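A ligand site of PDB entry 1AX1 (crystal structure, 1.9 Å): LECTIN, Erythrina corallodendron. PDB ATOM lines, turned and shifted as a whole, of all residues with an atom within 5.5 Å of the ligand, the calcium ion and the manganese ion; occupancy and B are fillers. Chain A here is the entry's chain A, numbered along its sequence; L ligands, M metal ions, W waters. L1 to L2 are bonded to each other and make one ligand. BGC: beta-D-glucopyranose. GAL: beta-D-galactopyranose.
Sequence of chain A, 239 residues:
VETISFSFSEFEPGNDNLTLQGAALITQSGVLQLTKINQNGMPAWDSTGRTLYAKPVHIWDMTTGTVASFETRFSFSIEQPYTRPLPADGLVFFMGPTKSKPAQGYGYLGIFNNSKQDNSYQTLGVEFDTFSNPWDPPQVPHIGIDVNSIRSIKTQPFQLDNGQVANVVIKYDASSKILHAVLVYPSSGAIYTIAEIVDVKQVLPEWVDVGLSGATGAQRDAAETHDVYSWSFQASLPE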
ATOM      1  N   PRO A  85     -23.622 -30.125  -0.895  1.00  0.00           N
ATOM      2  CA  PRO A  85     -24.573 -29.001  -0.927  1.00  0.00           C
ATOM      3  C   PRO A  85     -23.986 -27.786  -0.228  1.00  0.00           C
ATOM      4  O   PRO A  85     -22.862 -27.833   0.298  1.00  0.00           O
ATOM      5  CB  PRO A  85     -25.766 -29.558  -0.162  1.00  0.00           C
ATOM      6  CG  PRO A  85     -25.122 -30.427   0.857  1.00  0.00           C
ATOM      7  CD  PRO A  85     -24.067 -31.157   0.056  1.00  0.00           C
ATOM      8  N   LEU A  86     -24.716 -26.674  -0.262  1.00  0.00           N
ATOM      9  CA  LEU A  86     -24.261 -25.456   0.386  1.00  0.00           C
ATOM     10  C   LEU A  86     -24.122 -25.712   1.891  1.00  0.00           C
ATOM     11  O   LEU A  86     -24.917 -26.441   2.473  1.00  0.00           O
ATOM     12  CB  LEU A  86     -25.248 -24.316   0.142  1.00  0.00           C
ATOM     13  CG  LEU A  86     -25.498 -23.947  -1.318  1.00  0.00           C
ATOM     14  CD1 LEU A  86     -26.567 -22.882  -1.389  1.00  0.00           C
ATOM     15  CD2 LEU A  86     -24.206 -23.462  -1.957  1.00  0.00           C
ATOM     16  N   ALA A  88     -24.054 -24.943   6.048  1.00  0.00           N
ATOM     17  CA  ALA A  88     -25.022 -24.334   6.951  1.00  0.00           C
ATOM     18  C   ALA A  88     -24.664 -24.731   8.383  1.00  0.00           C
ATOM     19  O   ALA A  88     -23.892 -25.661   8.564  1.00  0.00           O
ATOM     20  CB  ALA A  88     -26.408 -24.840   6.594  1.00  0.00           C
ATOM     21  N   ASP A  89     -25.172 -24.030   9.410  1.00  0.00           N
ATOM     22  CA  ASP A  89     -26.072 -22.883   9.297  1.00  0.00           C
ATOM     23  C   ASP A  89     -25.469 -21.614   9.885  1.00  0.00           C
ATOM     24  O   ASP A  89     -25.881 -20.493   9.552  1.00  0.00           O
ATOM     25  CB  ASP A  89     -27.401 -23.162  10.002  1.00  0.00           C
ATOM     26  CG  ASP A  89     -28.440 -23.749   9.074  1.00  0.00           C
ATOM     27  OD1 ASP A  89     -29.034 -22.985   8.291  1.00  0.00           O
ATOM     28  OD2 ASP A  89     -28.640 -24.979   9.124  1.00  0.00           O
ATOM     29  N   TYR A 106     -30.813 -25.745  12.893  1.00  0.00           N
ATOM     30  CA  TYR A 106     -30.774 -25.271  11.513  1.00  0.00           C
ATOM     31  C   TYR A 106     -30.714 -23.745  11.441  1.00  0.00           C
ATOM     32  O   TYR A 106     -29.934 -23.121  12.172  1.00  0.00           O
ATOM     33  CB  TYR A 106     -31.974 -25.804  10.711  1.00  0.00           C
ATOM     34  CG  TYR A 106     -32.218 -27.275  10.911  1.00  0.00           C
ATOM     35  CD1 TYR A 106     -31.172 -28.190  10.830  1.00  0.00           C
ATOM     36  CD2 TYR A 106     -33.489 -27.752  11.214  1.00  0.00           C
ATOM     37  CE1 TYR A 106     -31.383 -29.546  11.073  1.00  0.00           C
ATOM     38  CE2 TYR A 106     -33.711 -29.090  11.463  1.00  0.00           C
ATOM     39  CZ  TYR A 106     -32.663 -29.984  11.389  1.00  0.00           C
ATOM     40  OH  TYR A 106     -32.901 -31.316  11.610  1.00  0.00           O
ATOM     41  N   GLY A 107     -31.517 -23.158  10.549  1.00  0.00           N
ATOM     42  CA  GLY A 107     -31.555 -21.723  10.363  1.00  0.00           C
ATOM     43  C   GLY A 107     -31.927 -20.930  11.595  1.00  0.00           C
ATOM     44  O   GLY A 107     -31.736 -19.716  11.636  1.00  0.00           O
ATOM     45  N   GLU A 127     -25.411 -12.840  15.190  1.00  0.00           N
ATOM     46  CA  GLU A 127     -25.158 -14.028  14.392  1.00  0.00           C
ATOM     47  C   GLU A 127     -24.086 -13.891  13.320  1.00  0.00           C
ATOM     48  O   GLU A 127     -23.740 -12.798  12.880  1.00  0.00           O
ATOM     49  CB  GLU A 127     -26.452 -14.486  13.737  1.00  0.00           C
ATOM     50  CG  GLU A 127     -27.026 -13.446  12.775  1.00  0.00           C
ATOM     51  CD  GLU A 127     -28.205 -13.944  11.971  1.00  0.00           C
ATOM     52  OE1 GLU A 127     -29.130 -14.515  12.561  1.00  0.00           O
ATOM     53  OE2 GLU A 127     -28.192 -13.758  10.736  1.00  0.00           O
ATOM     54  N   ASP A 129     -24.106 -15.905  10.236  1.00  0.00           N
ATOM     55  CA  ASP A 129     -24.961 -16.720   9.390  1.00  0.00           C
ATOM     56  C   ASP A 129     -24.338 -17.154   8.067  1.00  0.00           C
ATOM     57  O   ASP A 129     -24.044 -16.317   7.217  1.00  0.00           O
ATOM     58  CB  ASP A 129     -26.241 -15.924   9.140  1.00  0.00           C
ATOM     59  CG  ASP A 129     -27.396 -16.784   8.695  1.00  0.00           C
ATOM     60  OD1 ASP A 129     -27.203 -17.934   8.251  1.00  0.00           O
ATOM     61  OD2 ASP A 129     -28.536 -16.291   8.791  1.00  0.00           O
ATOM     62  N   THR A 130     -24.243 -18.459   7.868  1.00  0.00           N
ATOM     63  CA  THR A 130     -23.635 -19.009   6.658  1.00  0.00           C
ATOM     64  C   THR A 130     -24.596 -19.565   5.596  1.00  0.00           C
ATOM     65  O   THR A 130     -24.149 -19.939   4.507  1.00  0.00           O
ATOM     66  CB  THR A 130     -22.606 -20.102   6.996  1.00  0.00           C
ATOM     67  OG1 THR A 130     -23.249 -21.173   7.701  1.00  0.00           O
ATOM     68  CG2 THR A 130     -21.484 -19.533   7.869  1.00  0.00           C
ATOM     69  N   PHE A 131     -25.886 -19.638   5.909  1.00  0.00           N
ATOM     70  CA  PHE A 131     -26.863 -20.147   4.948  1.00  0.00           C
ATOM     71  C   PHE A 131     -28.009 -19.167   4.784  1.00  0.00           C
ATOM     72  O   PHE A 131     -28.593 -18.711   5.764  1.00  0.00           O
ATOM     73  CB  PHE A 131     -27.401 -21.516   5.384  1.00  0.00           C
ATOM     74  CG  PHE A 131     -28.390 -22.100   4.411  1.00  0.00           C
ATOM     75  CD1 PHE A 131     -29.746 -21.805   4.507  1.00  0.00           C
ATOM     76  CD2 PHE A 131     -27.958 -22.917   3.365  1.00  0.00           C
ATOM     77  CE1 PHE A 131     -30.666 -22.302   3.596  1.00  0.00           C
ATOM     78  CE2 PHE A 131     -28.868 -23.432   2.448  1.00  0.00           C
ATOM     79  CZ  PHE A 131     -30.228 -23.115   2.562  1.00  0.00           C
ATOM     80  N   SER A 132     -28.351 -18.887   3.536  1.00  0.00           N
ATOM     81  CA  SER A 132     -29.423 -17.953   3.215  1.00  0.00           C
ATOM     82  C   SER A 132     -30.835 -18.571   3.225  1.00  0.00           C
ATOM     83  O   SER A 132     -31.230 -19.251   2.274  1.00  0.00           O
ATOM     84  CB  SER A 132     -29.126 -17.268   1.876  1.00  0.00           C
ATOM     85  OG  SER A 132     -29.976 -16.158   1.674  1.00  0.00           O
ATOM     86  N   ASN A 133     -31.557 -18.361   4.330  1.00  0.00           N
ATOM     87  CA  ASN A 133     -32.931 -18.845   4.493  1.00  0.00           C
ATOM     88  C   ASN A 133     -33.852 -17.809   3.844  1.00  0.00           C
ATOM     89  O   ASN A 133     -33.405 -16.742   3.439  1.00  0.00           O
ATOM     90  CB  ASN A 133     -33.268 -18.987   5.981  1.00  0.00           C
ATOM     91  CG  ASN A 133     -32.404 -20.021   6.678  1.00  0.00           C
ATOM     92  OD1 ASN A 133     -31.378 -19.698   7.263  1.00  0.00           O
ATOM     93  ND2 ASN A 133     -32.833 -21.271   6.637  1.00  0.00           N
ATOM     94  N   TRP A 135     -35.860 -15.776   5.088  1.00  0.00           N
ATOM     95  CA  TRP A 135     -35.907 -14.538   5.872  1.00  0.00           C
ATOM     96  C   TRP A 135     -34.570 -13.781   5.849  1.00  0.00           C
ATOM     97  O   TRP A 135     -34.456 -12.697   6.423  1.00  0.00           O
ATOM     98  CB  TRP A 135     -36.294 -14.846   7.324  1.00  0.00           C
ATOM     99  CG  TRP A 135     -35.368 -15.837   7.976  1.00  0.00           C
ATOM    100  CD1 TRP A 135     -34.093 -15.601   8.439  1.00  0.00           C
ATOM    101  CD2 TRP A 135     -35.638 -17.220   8.237  1.00  0.00           C
ATOM    102  NE1 TRP A 135     -33.561 -16.753   8.972  1.00  0.00           N
ATOM    103  CE2 TRP A 135     -34.489 -17.761   8.850  1.00  0.00           C
ATOM    104  CE3 TRP A 135     -36.732 -18.050   7.995  1.00  0.00           C
ATOM    105  CZ2 TRP A 135     -34.401 -19.110   9.247  1.00  0.00           C
ATOM    106  CZ3 TRP A 135     -36.658 -19.399   8.383  1.00  0.00           C
ATOM    107  CH2 TRP A 135     -35.502 -19.907   8.995  1.00  0.00           C
ATOM    108  N   ASP A 136     -33.560 -14.362   5.213  1.00  0.00           N
ATOM    109  CA  ASP A 136     -32.230 -13.772   5.139  1.00  0.00           C
ATOM    110  C   ASP A 136     -31.955 -12.980   3.877  1.00  0.00           C
ATOM    111  O   ASP A 136     -32.654 -13.123   2.867  1.00  0.00           O
ATOM    112  CB  ASP A 136     -31.169 -14.871   5.168  1.00  0.00           C
ATOM    113  CG  ASP A 136     -30.925 -15.412   6.545  1.00  0.00           C
ATOM    114  OD1 ASP A 136     -30.908 -14.602   7.495  1.00  0.00           O
ATOM    115  OD2 ASP A 136     -30.731 -16.643   6.674  1.00  0.00           O
ATOM    116  N   PRO A 137     -30.954 -12.078   3.928  1.00  0.00           N
ATOM    117  CA  PRO A 137     -30.612 -11.324   2.733  1.00  0.00           C
ATOM    118  C   PRO A 137     -29.934 -12.381   1.844  1.00  0.00           C
ATOM    119  O   PRO A 137     -29.538 -13.446   2.342  1.00  0.00           O
ATOM    120  CB  PRO A 137     -29.612 -10.281   3.258  1.00  0.00           C
ATOM    121  CG  PRO A 137     -29.080 -10.886   4.516  1.00  0.00           C
ATOM    122  CD  PRO A 137     -30.306 -11.504   5.118  1.00  0.00           C
ATOM    123  N   HIS A 142     -23.027 -13.555   6.609  1.00  0.00           N
ATOM    124  CA  HIS A 142     -23.323 -12.203   7.062  1.00  0.00           C
ATOM    125  C   HIS A 142     -23.428 -12.151   8.578  1.00  0.00           C
ATOM    126  O   HIS A 142     -23.741 -13.149   9.234  1.00  0.00           O
ATOM    127  CB  HIS A 142     -24.596 -11.633   6.416  1.00  0.00           C
ATOM    128  CG  HIS A 142     -25.849 -12.417   6.718  1.00  0.00           C
ATOM    129  ND1 HIS A 142     -26.398 -13.334   5.855  1.00  0.00           N
ATOM    130  CD2 HIS A 142     -26.657 -12.401   7.802  1.00  0.00           C
ATOM    131  CE1 HIS A 142     -27.505 -13.841   6.428  1.00  0.00           C
ATOM    132  NE2 HIS A 142     -27.697 -13.303   7.608  1.00  0.00           N
ATOM    133  N   ILE A 150     -35.143 -14.159  14.341  1.00  0.00           N
ATOM    134  CA  ILE A 150     -34.042 -14.643  13.516  1.00  0.00           C
ATOM    135  C   ILE A 150     -33.894 -13.704  12.300  1.00  0.00           C
ATOM    136  O   ILE A 150     -32.876 -13.711  11.609  1.00  0.00           O
ATOM    137  CB  ILE A 150     -34.266 -16.130  13.079  1.00  0.00           C
ATOM    138  CG1 ILE A 150     -32.978 -16.712  12.492  1.00  0.00           C
ATOM    139  CG2 ILE A 150     -35.447 -16.247  12.131  1.00  0.00           C
ATOM    140  CD1 ILE A 150     -31.839 -16.853  13.502  1.00  0.00           C
ATOM    141  N   SER A 152     -32.882 -10.574  11.261  1.00  0.00           N
ATOM    142  CA  SER A 152     -32.059  -9.482  11.775  1.00  0.00           C
ATOM    143  C   SER A 152     -32.591  -8.086  11.495  1.00  0.00           C
ATOM    144  O   SER A 152     -33.201  -7.851  10.457  1.00  0.00           O
ATOM    145  CB  SER A 152     -30.649  -9.581  11.188  1.00  0.00           C
ATOM    146  OG  SER A 152     -30.149 -10.886  11.331  1.00  0.00           O
ATOM    147  N   THR A 155     -27.991  -6.135   8.986  1.00  0.00           N
ATOM    148  CA  THR A 155     -27.128  -7.181   8.440  1.00  0.00           C
ATOM    149  C   THR A 155     -25.862  -6.614   7.788  1.00  0.00           C
ATOM    150  O   THR A 155     -25.866  -5.489   7.273  1.00  0.00           O
ATOM    151  CB  THR A 155     -27.948  -8.068   7.443  1.00  0.00           C
ATOM    152  OG1 THR A 155     -28.351  -9.274   8.095  1.00  0.00           O
ATOM    153  CG2 THR A 155     -27.184  -8.383   6.197  1.00  0.00           C
ATOM    154  N   THR A 216     -25.654 -27.031  12.363  1.00  0.00           N
ATOM    155  CA  THR A 216     -25.367 -27.488  11.000  1.00  0.00           C
ATOM    156  C   THR A 216     -26.719 -27.762  10.302  1.00  0.00           C
ATOM    157  O   THR A 216     -27.767 -27.811  10.958  1.00  0.00           O
ATOM    158  CB  THR A 216     -24.412 -28.703  10.941  1.00  0.00           C
ATOM    159  OG1 THR A 216     -24.908 -29.775  11.748  1.00  0.00           O
ATOM    160  CG2 THR A 216     -23.032 -28.286  11.429  1.00  0.00           C
ATOM    161  N   GLY A 217     -26.681 -27.914   8.981  1.00  0.00           N
ATOM    162  CA  GLY A 217     -27.875 -28.094   8.172  1.00  0.00           C
ATOM    163  C   GLY A 217     -28.851 -29.248   8.324  1.00  0.00           C
ATOM    164  O   GLY A 217     -28.573 -30.258   8.976  1.00  0.00           O
ATOM    165  N   ALA A 218     -29.983 -29.081   7.637  1.00  0.00           N
ATOM    166  CA  ALA A 218     -31.100 -30.039   7.631  1.00  0.00           C
ATOM    167  C   ALA A 218     -31.009 -31.205   6.635  1.00  0.00           C
ATOM    168  O   ALA A 218     -31.900 -32.048   6.592  1.00  0.00           O
ATOM    169  CB  ALA A 218     -32.405 -29.288   7.432  1.00  0.00           C
ATOM    170  N   GLN A 219     -29.964 -31.248   5.814  1.00  0.00           N
ATOM    171  CA  GLN A 219     -29.794 -32.341   4.855  1.00  0.00           C
ATOM    172  C   GLN A 219     -28.354 -32.841   4.866  1.00  0.00           C
ATOM    173  O   GLN A 219     -27.443 -32.119   5.290  1.00  0.00           O
ATOM    174  CB  GLN A 219     -30.220 -31.928   3.445  1.00  0.00           C
ATOM    175  CG  GLN A 219     -29.264 -30.987   2.766  1.00  0.00           C
ATOM    176  CD  GLN A 219     -29.693 -30.691   1.341  1.00  0.00           C
ATOM    177  OE1 GLN A 219     -29.060 -31.139   0.392  1.00  0.00           O
ATOM    178  NE2 GLN A 219     -30.768 -29.924   1.201  1.00  0.00           N
ATOM    179  N   ALA A 222     -24.763 -30.828   4.534  1.00  0.00           N
ATOM    180  CA  ALA A 222     -24.937 -29.379   4.564  1.00  0.00           C
ATOM    181  C   ALA A 222     -24.382 -29.049   5.950  1.00  0.00           C
ATOM    182  O   ALA A 222     -25.132 -28.921   6.917  1.00  0.00           O
ATOM    183  CB  ALA A 222     -26.417 -28.999   4.456  1.00  0.00           C
HETATM  184  C2  BGC L   1     -34.303 -29.961   2.775  1.00  0.00           C
HETATM  185  C3  BGC L   1     -33.670 -29.166   3.908  1.00  0.00           C
HETATM  186  C4  BGC L   1     -34.371 -27.815   4.071  1.00  0.00           C
HETATM  187  C5  BGC L   1     -35.878 -28.032   4.212  1.00  0.00           C
HETATM  188  C6  BGC L   1     -36.674 -26.746   4.300  1.00  0.00           C
HETATM  189  C1  BGC L   1     -35.804 -30.068   3.003  1.00  0.00           C
HETATM  190  O1  BGC L   1     -36.391 -30.710   1.923  1.00  0.00           O
HETATM  191  O2  BGC L   1     -33.722 -31.257   2.714  1.00  0.00           O
HETATM  192  O3  BGC L   1     -32.290 -28.975   3.623  1.00  0.00           O
HETATM  193  O4  BGC L   1     -33.896 -27.150   5.261  1.00  0.00           O
HETATM  194  O5  BGC L   1     -36.387 -28.764   3.088  1.00  0.00           O
HETATM  195  O6  BGC L   1     -36.154 -25.757   3.413  1.00  0.00           O
HETATM  196  C1  GAL L   2     -32.887 -26.204   5.115  1.00  0.00           C
HETATM  197  C2  GAL L   2     -32.824 -25.373   6.405  1.00  0.00           C
HETATM  198  C3  GAL L   2     -31.608 -24.435   6.374  1.00  0.00           C
HETATM  199  C4  GAL L   2     -30.343 -25.274   6.140  1.00  0.00           C
HETATM  200  C5  GAL L   2     -30.524 -26.034   4.831  1.00  0.00           C
HETATM  201  C6  GAL L   2     -29.323 -26.887   4.483  1.00  0.00           C
HETATM  202  O2  GAL L   2     -34.016 -24.613   6.556  1.00  0.00           O
HETATM  203  O3  GAL L   2     -31.501 -23.743   7.606  1.00  0.00           O
HETATM  204  O4  GAL L   2     -30.153 -26.182   7.209  1.00  0.00           O
HETATM  205  O5  GAL L   2     -31.656 -26.920   4.922  1.00  0.00           O
HETATM  206  O6  GAL L   2     -29.541 -27.570   3.263  1.00  0.00           O
HETATM  207 CA    CA M   1     -29.548 -18.341   7.853  1.00  0.00          CA
HETATM  208 MN    MN M   2     -29.302 -14.264   8.936  1.00  0.00          MN
HETATM  209  O   HOH W   1     -30.188 -12.294   9.033  1.00  0.00           O
HETATM  210  O   HOH W   2     -35.007 -22.475   5.023  1.00  0.00           O
HETATM  211  O   HOH W   3     -34.143 -23.382   2.472  1.00  0.00           O
HETATM  212  O   HOH W   4     -31.355 -26.255   0.973  1.00  0.00           O
HETATM  213  O   HOH W   5     -30.777 -17.929   9.811  1.00  0.00           O
HETATM  214  O   HOH W   6     -30.899 -15.113  10.529  1.00  0.00           O
HETATM  215  O   HOH W   7     -33.668 -33.350   4.575  1.00  0.00           O
HETATM  216  O   HOH W   8     -36.143 -26.007   8.417  1.00  0.00           O
HETATM  217  O   HOH W   9     -28.723 -20.292   8.586  1.00  0.00           O
HETATM  218  O   HOH W  10     -27.534 -27.224   1.647  1.00  0.00           O
HETATM  219  O   HOH W  11     -34.375 -23.461   9.230  1.00  0.00           O
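The backbone NH (N) of Gly 107 sits at hydrogen-bond distance from the side-chain carboxylate (OD1) of Asp 89.
The backbone carbonyl oxygen (O) of Asp 89 sits at hydrogen-bond distance from the backbone NH (N) of Thr 130, 3.1 Å away.
The backbone NH of Gly 217 lies within hydrogen-bond range of the backbone carbonyl oxygen of Ala 222.
The calcium ion is bound by water W9 (2.2 Å), O of Phe 131 (2.3 Å), water W5 (2.3 Å), OD1 of Asn 133 (2.4 Å), OD2 of Asp 136 (2.4 Å), OD1 of Asp 129 (2.4 Å) and OD2 of Asp 129 (2.5 Å).
The calcium ion has seven donor atoms within binding distance.
Water W5 bridges O of Gly 107 and NE1 of Trp 135.
Water W6 lies within hydrogen-bond range of the backbone carbonyl oxygen (O) of Ile 150, the side-chain carboxylate (OE1) of Glu 127 and the indole nitrogen (NE1) of Trp 135.
Water W10 bridges O6 of GAL L2 (2.6 Å) and O of Leu 86 (2.9 Å).
Water W7 lies within hydrogen-bond range of an oxygen (O2) of BGC L1 (2.8 Å) and the backbone carbonyl oxygen (O) of Ala 218 (3.0 Å).
Water W2 bridges O2 of GAL L2 (2.8 Å) and ND2 of Asn 133 (3.0 Å).
Water W11 lies within hydrogen-bond range of an oxygen (O2) of GAL L2 (2.9 Å) and the backbone NH of Gly 107 (3.2 Å).
Merely in contact with the ligand: Ala 88 (3.98 Å), Tyr 106 (3.8 Å), Gly 217 (3.1 Å) and Ala 222 (3.6 Å).
Hydrophobic or aromatic side chains that line the ligand: Ala 88, Tyr 106, Phe 131, Ala 218 and Ala 222.
Of the 24 residues printed, 10 come within 4 Å of the ligand.
The nearest printed residue that does not touch the manganese ion is Ser 152 (4.2 Å).
Four residues have an atom within 4 Å of the calcium ion: Asp 129, Phe 131, Asn 133 and Asp 136.
The nearest printed residue that does not touch the calcium ion is Trp 135 (4.5 Å).
ND2 of Asn 133 is in hydrogen-bond range of O3 of GAL L2, at 3.0 Å.
The side-chain carboxylate (OD1) of Asp 89 sits at hydrogen-bond distance from an oxygen (O3) of GAL L2 (2.7 Å).
N of Ala 218 lies within hydrogen-bond range of O4 of GAL L2 (2.9 Å).
O3 of GAL L2 sits at hydrogen-bond distance from N of Gly 107 (3.0 Å).
NE2 of Gln 219 is in hydrogen-bond range of O3 of BGC L1, 3.0 Å away.
The manganese ion is bound by water W1, the side-chain carboxylate of Asp 129, the side-chain carboxylate of Glu 127, the side-chain carboxylate of Asp 136, a ring nitrogen (NE2) of His 142 and water W6.
The manganese ion has six donor atoms within binding distance.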
